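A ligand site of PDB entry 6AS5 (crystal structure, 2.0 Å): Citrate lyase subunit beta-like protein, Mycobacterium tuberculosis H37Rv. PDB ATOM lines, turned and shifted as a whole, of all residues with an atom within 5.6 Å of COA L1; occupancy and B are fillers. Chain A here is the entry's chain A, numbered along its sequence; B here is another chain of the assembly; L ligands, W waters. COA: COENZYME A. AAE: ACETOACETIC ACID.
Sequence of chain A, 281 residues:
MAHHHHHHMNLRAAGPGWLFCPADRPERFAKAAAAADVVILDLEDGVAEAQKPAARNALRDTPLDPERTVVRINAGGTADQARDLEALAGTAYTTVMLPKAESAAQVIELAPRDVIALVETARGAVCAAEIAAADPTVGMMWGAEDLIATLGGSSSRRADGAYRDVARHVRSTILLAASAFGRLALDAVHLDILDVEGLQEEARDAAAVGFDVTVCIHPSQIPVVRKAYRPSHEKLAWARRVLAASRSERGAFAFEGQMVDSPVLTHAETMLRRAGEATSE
Merely in contact with COA L1: Met 259 of chain B (3.3 Å), Pro 22 (3.3 Å), Asp 42 (3.4 Å), Pro 219 (3.4 Å), Arg 72 (3.6 Å), Ala 252 of chain B (3.7 Å), Ala 32 (3.9 Å) and Gly 46 (3.99 Å).
Hydrophobic or aromatic side chains that line COA L1: Phe 20, Pro 22, Ala 32, Ile 217, His 218, Pro 219, Ala 252 of chain B and Met 259 of chain B.
14 residues have an atom within 4 Å of COA L1: Phe 20, Cys 21, Pro 22, Arg 28, Lys 31, Ala 32, Asp 42, Gly 46, Arg 72, Ile 217, His 218, Pro 219, Ala 252 of chain B and Met 259 of chain B.
The nearest printed residue that does not touch COA L1 is Asp 261 of chain B (4.1 Å).
NH1 of Arg 25 sits close to NH1 of Arg 28, at 2.5 Å.
The backbone carbonyl oxygen (O) of Leu 191 lies within hydrogen-bond range of the backbone NH (N) of Met 259 of chain B (2.7 Å).
The backbone NH of Asp 42 sits at hydrogen-bond distance from the backbone carbonyl oxygen of Cys 21, 3.0 Å away.
OD1 of Asp 42 lies within salt-bridge range of NE of Arg 72 (2.8 Å).
OD2 of Asp 42 sits at hydrogen-bond distance from N of Gly 46 (2.8 Å).
O of Gly 46 is in hydrogen-bond range of N of Ala 252 of chain B (2.9 Å).
A ring nitrogen (NE2) of His 218 is in hydrogen-bond range of an oxygen (O2A) of COA L1 (2.7 Å).
N8P of COA L1 sits at hydrogen-bond distance from O of Ile 217.
O5A of COA L1 lies within salt-bridge range of NH2 of Arg 28.
The backbone carbonyl oxygen (O) of Phe 20 lies within hydrogen-bond range of a nitrogen (N6A) of COA L1, 2.9 Å away.
The side-chain sulfur of Cys 21 is in hydrogen-bond range of a nitrogen (N1A) of COA L1, at 3.5 Å.
The side-chain amino group (NZ) of Lys 31 is in salt-bridge range of an oxygen (O9A) of COA L1 (3.5 Å).
O8 of AAE L2 lies close to NH1 of Arg 72, at 2.7 Å.
Water W1 lies within hydrogen-bond range of the side-chain carboxylate of Asp 261 of chain B, a sulfur (S1P) of COA L1 and the guanidinium group of Arg 72.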
ATOM      1  N   LEU A  19       2.161  24.442  15.838  1.00  0.00           N
ATOM      2  CA  LEU A  19       3.003  25.425  15.180  1.00  0.00           C
ATOM      3  C   LEU A  19       4.442  25.462  15.676  1.00  0.00           C
ATOM      4  O   LEU A  19       4.679  25.729  16.857  1.00  0.00           O
ATOM      5  CB  LEU A  19       2.407  26.825  15.350  1.00  0.00           C
ATOM      6  CG  LEU A  19       3.119  28.008  14.710  1.00  0.00           C
ATOM      7  CD1 LEU A  19       3.435  27.719  13.261  1.00  0.00           C
ATOM      8  CD2 LEU A  19       2.241  29.233  14.821  1.00  0.00           C
ATOM      9  N   PHE A  20       5.380  25.205  14.773  1.00  0.00           N
ATOM     10  CA  PHE A  20       6.806  25.413  15.062  1.00  0.00           C
ATOM     11  C   PHE A  20       7.128  26.897  15.144  1.00  0.00           C
ATOM     12  O   PHE A  20       6.701  27.693  14.310  1.00  0.00           O
ATOM     13  CB  PHE A  20       7.689  24.816  13.948  1.00  0.00           C
ATOM     14  CG  PHE A  20       8.099  23.382  14.169  1.00  0.00           C
ATOM     15  CD1 PHE A  20       8.895  23.034  15.249  1.00  0.00           C
ATOM     16  CD2 PHE A  20       7.725  22.401  13.268  1.00  0.00           C
ATOM     17  CE1 PHE A  20       9.290  21.707  15.443  1.00  0.00           C
ATOM     18  CE2 PHE A  20       8.116  21.078  13.455  1.00  0.00           C
ATOM     19  CZ  PHE A  20       8.894  20.742  14.539  1.00  0.00           C
ATOM     20  N   CYS A  21       7.933  27.272  16.135  1.00  0.00           N
ATOM     21  CA  CYS A  21       8.533  28.606  16.153  1.00  0.00           C
ATOM     22  C   CYS A  21       9.936  28.467  16.735  1.00  0.00           C
ATOM     23  O   CYS A  21      10.100  27.875  17.803  1.00  0.00           O
ATOM     24  CB  CYS A  21       7.711  29.567  16.990  1.00  0.00           C
ATOM     25  SG  CYS A  21       8.404  31.243  17.030  1.00  0.00           S
ATOM     26  N   PRO A  22      10.944  28.985  16.021  1.00  0.00           N
ATOM     27  CA  PRO A  22      12.355  28.870  16.418  1.00  0.00           C
ATOM     28  C   PRO A  22      12.562  29.534  17.774  1.00  0.00           C
ATOM     29  O   PRO A  22      12.043  30.628  17.989  1.00  0.00           O
ATOM     30  CB  PRO A  22      13.083  29.656  15.335  1.00  0.00           C
ATOM     31  CG  PRO A  22      12.165  29.654  14.153  1.00  0.00           C
ATOM     32  CD  PRO A  22      10.771  29.651  14.718  1.00  0.00           C
ATOM     33  N   ARG A  25      13.691  33.210  18.478  1.00  0.00           N
ATOM     34  CA  ARG A  25      12.789  34.275  18.037  1.00  0.00           C
ATOM     35  C   ARG A  25      11.664  34.548  19.037  1.00  0.00           C
ATOM     36  O   ARG A  25      10.495  34.450  18.698  1.00  0.00           O
ATOM     37  CB  ARG A  25      12.220  33.963  16.648  1.00  0.00           C
ATOM     38  CG  ARG A  25      13.232  34.049  15.513  1.00  0.00           C
ATOM     39  CD  ARG A  25      12.502  33.985  14.177  1.00  0.00           C
ATOM     40  NE  ARG A  25      13.373  34.067  13.009  1.00  0.00           N
ATOM     41  CZ  ARG A  25      13.559  35.168  12.278  1.00  0.00           C
ATOM     42  NH1 ARG A  25      12.932  36.301  12.576  1.00  0.00           N
ATOM     43  NH2 ARG A  25      14.380  35.122  11.236  1.00  0.00           N
ATOM     44  N   ARG A  28       8.325  36.459  18.767  1.00  0.00           N
ATOM     45  CA  ARG A  28       7.225  35.771  18.092  1.00  0.00           C
ATOM     46  C   ARG A  28       6.473  34.784  18.975  1.00  0.00           C
ATOM     47  O   ARG A  28       5.448  34.245  18.556  1.00  0.00           O
ATOM     48  CB  ARG A  28       7.744  34.966  16.889  1.00  0.00           C
ATOM     49  CG  ARG A  28       8.091  35.757  15.629  1.00  0.00           C
ATOM     50  CD  ARG A  28       8.605  34.791  14.558  1.00  0.00           C
ATOM     51  NE  ARG A  28       8.680  35.393  13.225  1.00  0.00           N
ATOM     52  CZ  ARG A  28       9.677  36.168  12.819  1.00  0.00           C
ATOM     53  NH1 ARG A  28      10.671  36.457  13.653  1.00  0.00           N
ATOM     54  NH2 ARG A  28       9.676  36.688  11.604  1.00  0.00           N
ATOM     55  N   LYS A  31       2.765  35.449  19.858  1.00  0.00           N
ATOM     56  CA  LYS A  31       1.976  35.372  18.623  1.00  0.00           C
ATOM     57  C   LYS A  31       1.754  33.910  18.267  1.00  0.00           C
ATOM     58  O   LYS A  31       0.659  33.503  17.907  1.00  0.00           O
ATOM     59  CB  LYS A  31       2.700  36.085  17.494  1.00  0.00           C
ATOM     60  CG  LYS A  31       2.041  35.924  16.147  1.00  0.00           C
ATOM     61  CD  LYS A  31       0.706  36.630  16.129  1.00  0.00           C
ATOM     62  CE  LYS A  31       0.060  36.529  14.764  1.00  0.00           C
ATOM     63  NZ  LYS A  31       0.974  37.019  13.687  1.00  0.00           N
ATOM     64  N   ALA A  32       2.826  33.128  18.361  1.00  0.00           N
ATOM     65  CA  ALA A  32       2.739  31.709  18.094  1.00  0.00           C
ATOM     66  C   ALA A  32       1.677  31.108  19.005  1.00  0.00           C
ATOM     67  O   ALA A  32       0.732  30.477  18.534  1.00  0.00           O
ATOM     68  CB  ALA A  32       4.100  31.052  18.315  1.00  0.00           C
ATOM     69  N   ASP A  42      11.408  25.492  19.109  1.00  0.00           N
ATOM     70  CA  ASP A  42      12.431  24.665  18.490  1.00  0.00           C
ATOM     71  C   ASP A  42      13.861  25.059  18.862  1.00  0.00           C
ATOM     72  O   ASP A  42      14.257  26.197  18.661  1.00  0.00           O
ATOM     73  CB  ASP A  42      12.290  24.680  16.973  1.00  0.00           C
ATOM     74  CG  ASP A  42      13.271  23.749  16.294  1.00  0.00           C
ATOM     75  OD1 ASP A  42      13.663  22.736  16.923  1.00  0.00           O
ATOM     76  OD2 ASP A  42      13.660  24.029  15.133  1.00  0.00           O
ATOM     77  N   ASP A  45      16.807  22.197  14.219  1.00  0.00           N
ATOM     78  CA  ASP A  45      17.207  22.691  12.904  1.00  0.00           C
ATOM     79  C   ASP A  45      16.781  24.116  12.620  1.00  0.00           C
ATOM     80  O   ASP A  45      17.410  24.799  11.823  1.00  0.00           O
ATOM     81  CB  ASP A  45      16.737  21.753  11.781  1.00  0.00           C
ATOM     82  CG  ASP A  45      17.457  20.424  11.803  1.00  0.00           C
ATOM     83  OD1 ASP A  45      18.430  20.316  12.581  1.00  0.00           O
ATOM     84  OD2 ASP A  45      17.073  19.505  11.054  1.00  0.00           O
ATOM     85  N   GLY A  46      15.726  24.575  13.287  1.00  0.00           N
ATOM     86  CA  GLY A  46      15.218  25.918  13.098  1.00  0.00           C
ATOM     87  C   GLY A  46      16.231  26.993  13.473  1.00  0.00           C
ATOM     88  O   GLY A  46      16.175  28.106  12.943  1.00  0.00           O
ATOM     89  N   ARG A  72      11.008  21.154  21.017  1.00  0.00           N
ATOM     90  CA  ARG A  72      11.846  20.239  20.240  1.00  0.00           C
ATOM     91  C   ARG A  72      13.304  20.411  20.619  1.00  0.00           C
ATOM     92  O   ARG A  72      13.905  21.464  20.346  1.00  0.00           O
ATOM     93  CB  ARG A  72      11.669  20.419  18.721  1.00  0.00           C
ATOM     94  CG  ARG A  72      12.446  19.368  17.913  1.00  0.00           C
ATOM     95  CD  ARG A  72      12.044  19.326  16.445  1.00  0.00           C
ATOM     96  NE  ARG A  72      12.759  20.349  15.697  1.00  0.00           N
ATOM     97  CZ  ARG A  72      12.917  20.361  14.374  1.00  0.00           C
ATOM     98  NH1 ARG A  72      12.422  19.398  13.615  1.00  0.00           N
ATOM     99  NH2 ARG A  72      13.598  21.363  13.827  1.00  0.00           N
ATOM    100  N   VAL A 189       5.255  18.550   8.222  1.00  0.00           N
ATOM    101  CA  VAL A 189       5.110  19.969   7.930  1.00  0.00           C
ATOM    102  C   VAL A 189       4.959  20.224   6.434  1.00  0.00           C
ATOM    103  O   VAL A 189       5.350  19.401   5.601  1.00  0.00           O
ATOM    104  CB  VAL A 189       6.321  20.739   8.445  1.00  0.00           C
ATOM    105  CG1 VAL A 189       6.371  20.699   9.966  1.00  0.00           C
ATOM    106  CG2 VAL A 189       7.619  20.185   7.822  1.00  0.00           C
ATOM    107  N   LEU A 191       6.135  22.793   3.766  1.00  0.00           N
ATOM    108  CA  LEU A 191       7.189  23.794   3.652  1.00  0.00           C
ATOM    109  C   LEU A 191       6.868  24.920   2.680  1.00  0.00           C
ATOM    110  O   LEU A 191       7.423  26.013   2.811  1.00  0.00           O
ATOM    111  CB  LEU A 191       8.511  23.134   3.248  1.00  0.00           C
ATOM    112  CG  LEU A 191       9.029  22.158   4.307  1.00  0.00           C
ATOM    113  CD1 LEU A 191      10.456  21.744   4.011  1.00  0.00           C
ATOM    114  CD2 LEU A 191       8.944  22.813   5.666  1.00  0.00           C
ATOM    115  N   ILE A 193       5.004  27.685   2.054  1.00  0.00           N
ATOM    116  CA  ILE A 193       4.158  28.559   2.859  1.00  0.00           C
ATOM    117  C   ILE A 193       2.871  29.000   2.167  1.00  0.00           C
ATOM    118  O   ILE A 193       1.816  28.984   2.781  1.00  0.00           O
ATOM    119  CB  ILE A 193       4.922  29.801   3.307  1.00  0.00           C
ATOM    120  CG1 ILE A 193       6.047  29.395   4.266  1.00  0.00           C
ATOM    121  CG2 ILE A 193       3.972  30.780   3.963  1.00  0.00           C
ATOM    122  CD1 ILE A 193       7.050  30.501   4.562  1.00  0.00           C
ATOM    123  N   ILE A 217       4.264  25.439   9.915  1.00  0.00           N
ATOM    124  CA  ILE A 217       5.475  26.223  10.124  1.00  0.00           C
ATOM    125  C   ILE A 217       5.254  27.742  10.017  1.00  0.00           C
ATOM    126  O   ILE A 217       6.185  28.528  10.204  1.00  0.00           O
ATOM    127  CB  ILE A 217       6.682  25.721   9.282  1.00  0.00           C
ATOM    128  CG1 ILE A 217       6.308  25.480   7.824  1.00  0.00           C
ATOM    129  CG2 ILE A 217       7.212  24.398   9.867  1.00  0.00           C
ATOM    130  CD1 ILE A 217       5.869  26.715   7.066  1.00  0.00           C
ATOM    131  N   HIS A 218       4.016  28.150   9.749  1.00  0.00           N
ATOM    132  CA  HIS A 218       3.670  29.561   9.584  1.00  0.00           C
ATOM    133  C   HIS A 218       2.245  29.733  10.099  1.00  0.00           C
ATOM    134  O   HIS A 218       1.388  28.878   9.840  1.00  0.00           O
ATOM    135  CB  HIS A 218       3.792  29.958   8.105  1.00  0.00           C
ATOM    136  CG  HIS A 218       3.735  31.443   7.849  1.00  0.00           C
ATOM    137  ND1 HIS A 218       2.560  32.157   7.803  1.00  0.00           N
ATOM    138  CD2 HIS A 218       4.725  32.332   7.588  1.00  0.00           C
ATOM    139  CE1 HIS A 218       2.823  33.428   7.552  1.00  0.00           C
ATOM    140  NE2 HIS A 218       4.133  33.553   7.414  1.00  0.00           N
ATOM    141  N   PRO A 219       1.973  30.816  10.832  1.00  0.00           N
ATOM    142  CA  PRO A 219       0.674  30.902  11.511  1.00  0.00           C
ATOM    143  C   PRO A 219      -0.485  30.997  10.534  1.00  0.00           C
ATOM    144  O   PRO A 219      -1.623  30.677  10.884  1.00  0.00           O
ATOM    145  CB  PRO A 219       0.786  32.188  12.346  1.00  0.00           C
ATOM    146  CG  PRO A 219       1.894  32.975  11.718  1.00  0.00           C
ATOM    147  CD  PRO A 219       2.843  31.961  11.146  1.00  0.00           C
ATOM    148  N   ALA B 252      16.445  28.870  10.198  1.00  0.00           N
ATOM    149  CA  ALA B 252      15.342  28.665   9.254  1.00  0.00           C
ATOM    150  C   ALA B 252      14.976  29.976   8.575  1.00  0.00           C
ATOM    151  O   ALA B 252      14.795  30.990   9.240  1.00  0.00           O
ATOM    152  CB  ALA B 252      14.137  28.085   9.966  1.00  0.00           C
ATOM    153  N   PHE B 253      14.884  29.950   7.254  1.00  0.00           N
ATOM    154  CA  PHE B 253      14.436  31.130   6.531  1.00  0.00           C
ATOM    155  C   PHE B 253      13.507  30.730   5.405  1.00  0.00           C
ATOM    156  O   PHE B 253      13.361  29.557   5.082  1.00  0.00           O
ATOM    157  CB  PHE B 253      15.624  31.918   5.966  1.00  0.00           C
ATOM    158  CG  PHE B 253      16.488  31.136   5.015  1.00  0.00           C
ATOM    159  CD1 PHE B 253      16.407  31.367   3.650  1.00  0.00           C
ATOM    160  CD2 PHE B 253      17.362  30.170   5.485  1.00  0.00           C
ATOM    161  CE1 PHE B 253      17.209  30.645   2.772  1.00  0.00           C
ATOM    162  CE2 PHE B 253      18.156  29.452   4.614  1.00  0.00           C
ATOM    163  CZ  PHE B 253      18.085  29.686   3.258  1.00  0.00           C
ATOM    164  N   ALA B 254      12.884  31.735   4.802  1.00  0.00           N
ATOM    165  CA  ALA B 254      12.027  31.514   3.665  1.00  0.00           C
ATOM    166  C   ALA B 254      12.739  31.918   2.376  1.00  0.00           C
ATOM    167  O   ALA B 254      13.361  32.977   2.291  1.00  0.00           O
ATOM    168  CB  ALA B 254      10.735  32.287   3.826  1.00  0.00           C
ATOM    169  N   MET B 259       9.778  27.338   3.233  1.00  0.00           N
ATOM    170  CA  MET B 259      10.559  27.284   4.464  1.00  0.00           C
ATOM    171  C   MET B 259      11.801  26.470   4.132  1.00  0.00           C
ATOM    172  O   MET B 259      11.700  25.350   3.650  1.00  0.00           O
ATOM    173  CB  MET B 259       9.750  26.621   5.580  1.00  0.00           C
ATOM    174  CG  MET B 259      10.197  26.943   7.014  1.00  0.00           C
ATOM    175  SD  MET B 259      11.757  26.194   7.541  1.00  0.00           S
ATOM    176  CE  MET B 259      11.337  24.468   7.705  1.00  0.00           C
ATOM    177  N   ASP B 261      15.483  24.900   5.718  1.00  0.00           N
ATOM    178  CA  ASP B 261      16.500  24.710   6.760  1.00  0.00           C
ATOM    179  C   ASP B 261      17.457  23.545   6.463  1.00  0.00           C
ATOM    180  O   ASP B 261      17.388  22.940   5.389  1.00  0.00           O
ATOM    181  CB  ASP B 261      15.875  24.587   8.164  1.00  0.00           C
ATOM    182  CG  ASP B 261      15.100  23.298   8.374  1.00  0.00           C
ATOM    183  OD1 ASP B 261      15.147  22.388   7.507  1.00  0.00           O
ATOM    184  OD2 ASP B 261      14.433  23.183   9.425  1.00  0.00           O
HETATM  185  N1A COA L   1       5.928  31.644  14.604  1.00  0.00           N
HETATM  186  C2A COA L   1       5.350  32.789  15.002  1.00  0.00           C
HETATM  187  N3A COA L   1       5.080  33.788  14.129  1.00  0.00           N
HETATM  188  C4A COA L   1       5.391  33.650  12.823  1.00  0.00           C
HETATM  189  C5A COA L   1       5.993  32.479  12.369  1.00  0.00           C
HETATM  190  C6A COA L   1       6.249  31.461  13.302  1.00  0.00           C
HETATM  191  N6A COA L   1       6.889  30.194  12.829  1.00  0.00           N
HETATM  192  N7A COA L   1       6.186  32.607  11.040  1.00  0.00           N
HETATM  193  C8A COA L   1       5.732  33.812  10.677  1.00  0.00           C
HETATM  194  N9A COA L   1       5.251  34.452  11.751  1.00  0.00           N
HETATM  195  C1B COA L   1       4.654  35.767  11.786  1.00  0.00           C
HETATM  196  C2B COA L   1       5.592  36.873  11.723  1.00  0.00           C
HETATM  197  O2B COA L   1       5.933  37.262  13.009  1.00  0.00           O
HETATM  198  C3B COA L   1       4.812  37.919  11.139  1.00  0.00           C
HETATM  199  O3B COA L   1       4.004  38.418  12.147  1.00  0.00           O
HETATM  200  P3B COA L   1       3.658  39.936  12.172  1.00  0.00           P
HETATM  201  O7A COA L   1       3.569  40.442  10.744  1.00  0.00           O
HETATM  202  O8A COA L   1       4.754  40.656  12.923  1.00  0.00           O
HETATM  203  O9A COA L   1       2.321  40.150  12.851  1.00  0.00           O
HETATM  204  C4B COA L   1       3.976  37.233  10.167  1.00  0.00           C
HETATM  205  O4B COA L   1       3.836  35.888  10.672  1.00  0.00           O
HETATM  206  C5B COA L   1       4.591  37.226   8.839  1.00  0.00           C
HETATM  207  O5B COA L   1       5.798  36.601   8.677  1.00  0.00           O
HETATM  208  P1A COA L   1       6.364  36.287   7.276  1.00  0.00           P
HETATM  209  O1A COA L   1       6.959  37.529   6.711  1.00  0.00           O
HETATM  210  O2A COA L   1       5.276  35.754   6.382  1.00  0.00           O
HETATM  211  O3A COA L   1       7.454  35.186   7.385  1.00  0.00           O
HETATM  212  P2A COA L   1       8.919  35.520   7.881  1.00  0.00           P
HETATM  213  O4A COA L   1       9.814  35.811   6.709  1.00  0.00           O
HETATM  214  O5A COA L   1       8.862  36.641   8.867  1.00  0.00           O
HETATM  215  O6A COA L   1       9.474  34.249   8.567  1.00  0.00           O
HETATM  216  CBP COA L   1      10.005  31.896   8.677  1.00  0.00           C
HETATM  217  CCP COA L   1       9.373  33.046   7.899  1.00  0.00           C
HETATM  218  CDP COA L   1      11.380  32.314   9.185  1.00  0.00           C
HETATM  219  CEP COA L   1      10.091  30.630   7.855  1.00  0.00           C
HETATM  220  CAP COA L   1       9.031  31.632   9.856  1.00  0.00           C
HETATM  221  OAP COA L   1       7.814  31.340   9.270  1.00  0.00           O
HETATM  222  C9P COA L   1       9.439  30.444  10.701  1.00  0.00           C
HETATM  223  O9P COA L   1      10.315  30.543  11.563  1.00  0.00           O
HETATM  224  N8P COA L   1       8.792  29.198  10.412  1.00  0.00           N
HETATM  225  C7P COA L   1       9.106  27.970  11.149  1.00  0.00           C
HETATM  226  C6P COA L   1      10.552  27.572  11.181  1.00  0.00           C
HETATM  227  C5P COA L   1      10.852  26.388  12.059  1.00  0.00           C
HETATM  228  O5P COA L   1      10.572  26.406  13.270  1.00  0.00           O
HETATM  229  N4P COA L   1      11.467  25.233  11.478  1.00  0.00           N
HETATM  230  C3P COA L   1      11.719  24.143  12.365  1.00  0.00           C
HETATM  231  C2P COA L   1      10.923  22.883  12.053  1.00  0.00           C
HETATM  232  S1P COA L   1      10.480  22.667  10.334  1.00  0.00           S
HETATM  233  O1  AAE L   2      11.229  16.762   7.363  1.00  0.00           O
HETATM  234  C2  AAE L   2      11.895  17.326   8.264  1.00  0.00           C
HETATM  235  O3  AAE L   2      13.041  16.896   8.566  1.00  0.00           O
HETATM  236  C4  AAE L   2      11.323  18.526   8.971  1.00  0.00           C
HETATM  237  C5  AAE L   2      11.031  18.480  10.434  1.00  0.00           C
HETATM  238  O8  AAE L   2      11.904  18.195  11.239  1.00  0.00           O
HETATM  239  C9  AAE L   2       9.654  18.786  10.933  1.00  0.00           C
HETATM  240  O   HOH W   1      13.283  21.495  10.696  1.00  0.00           O
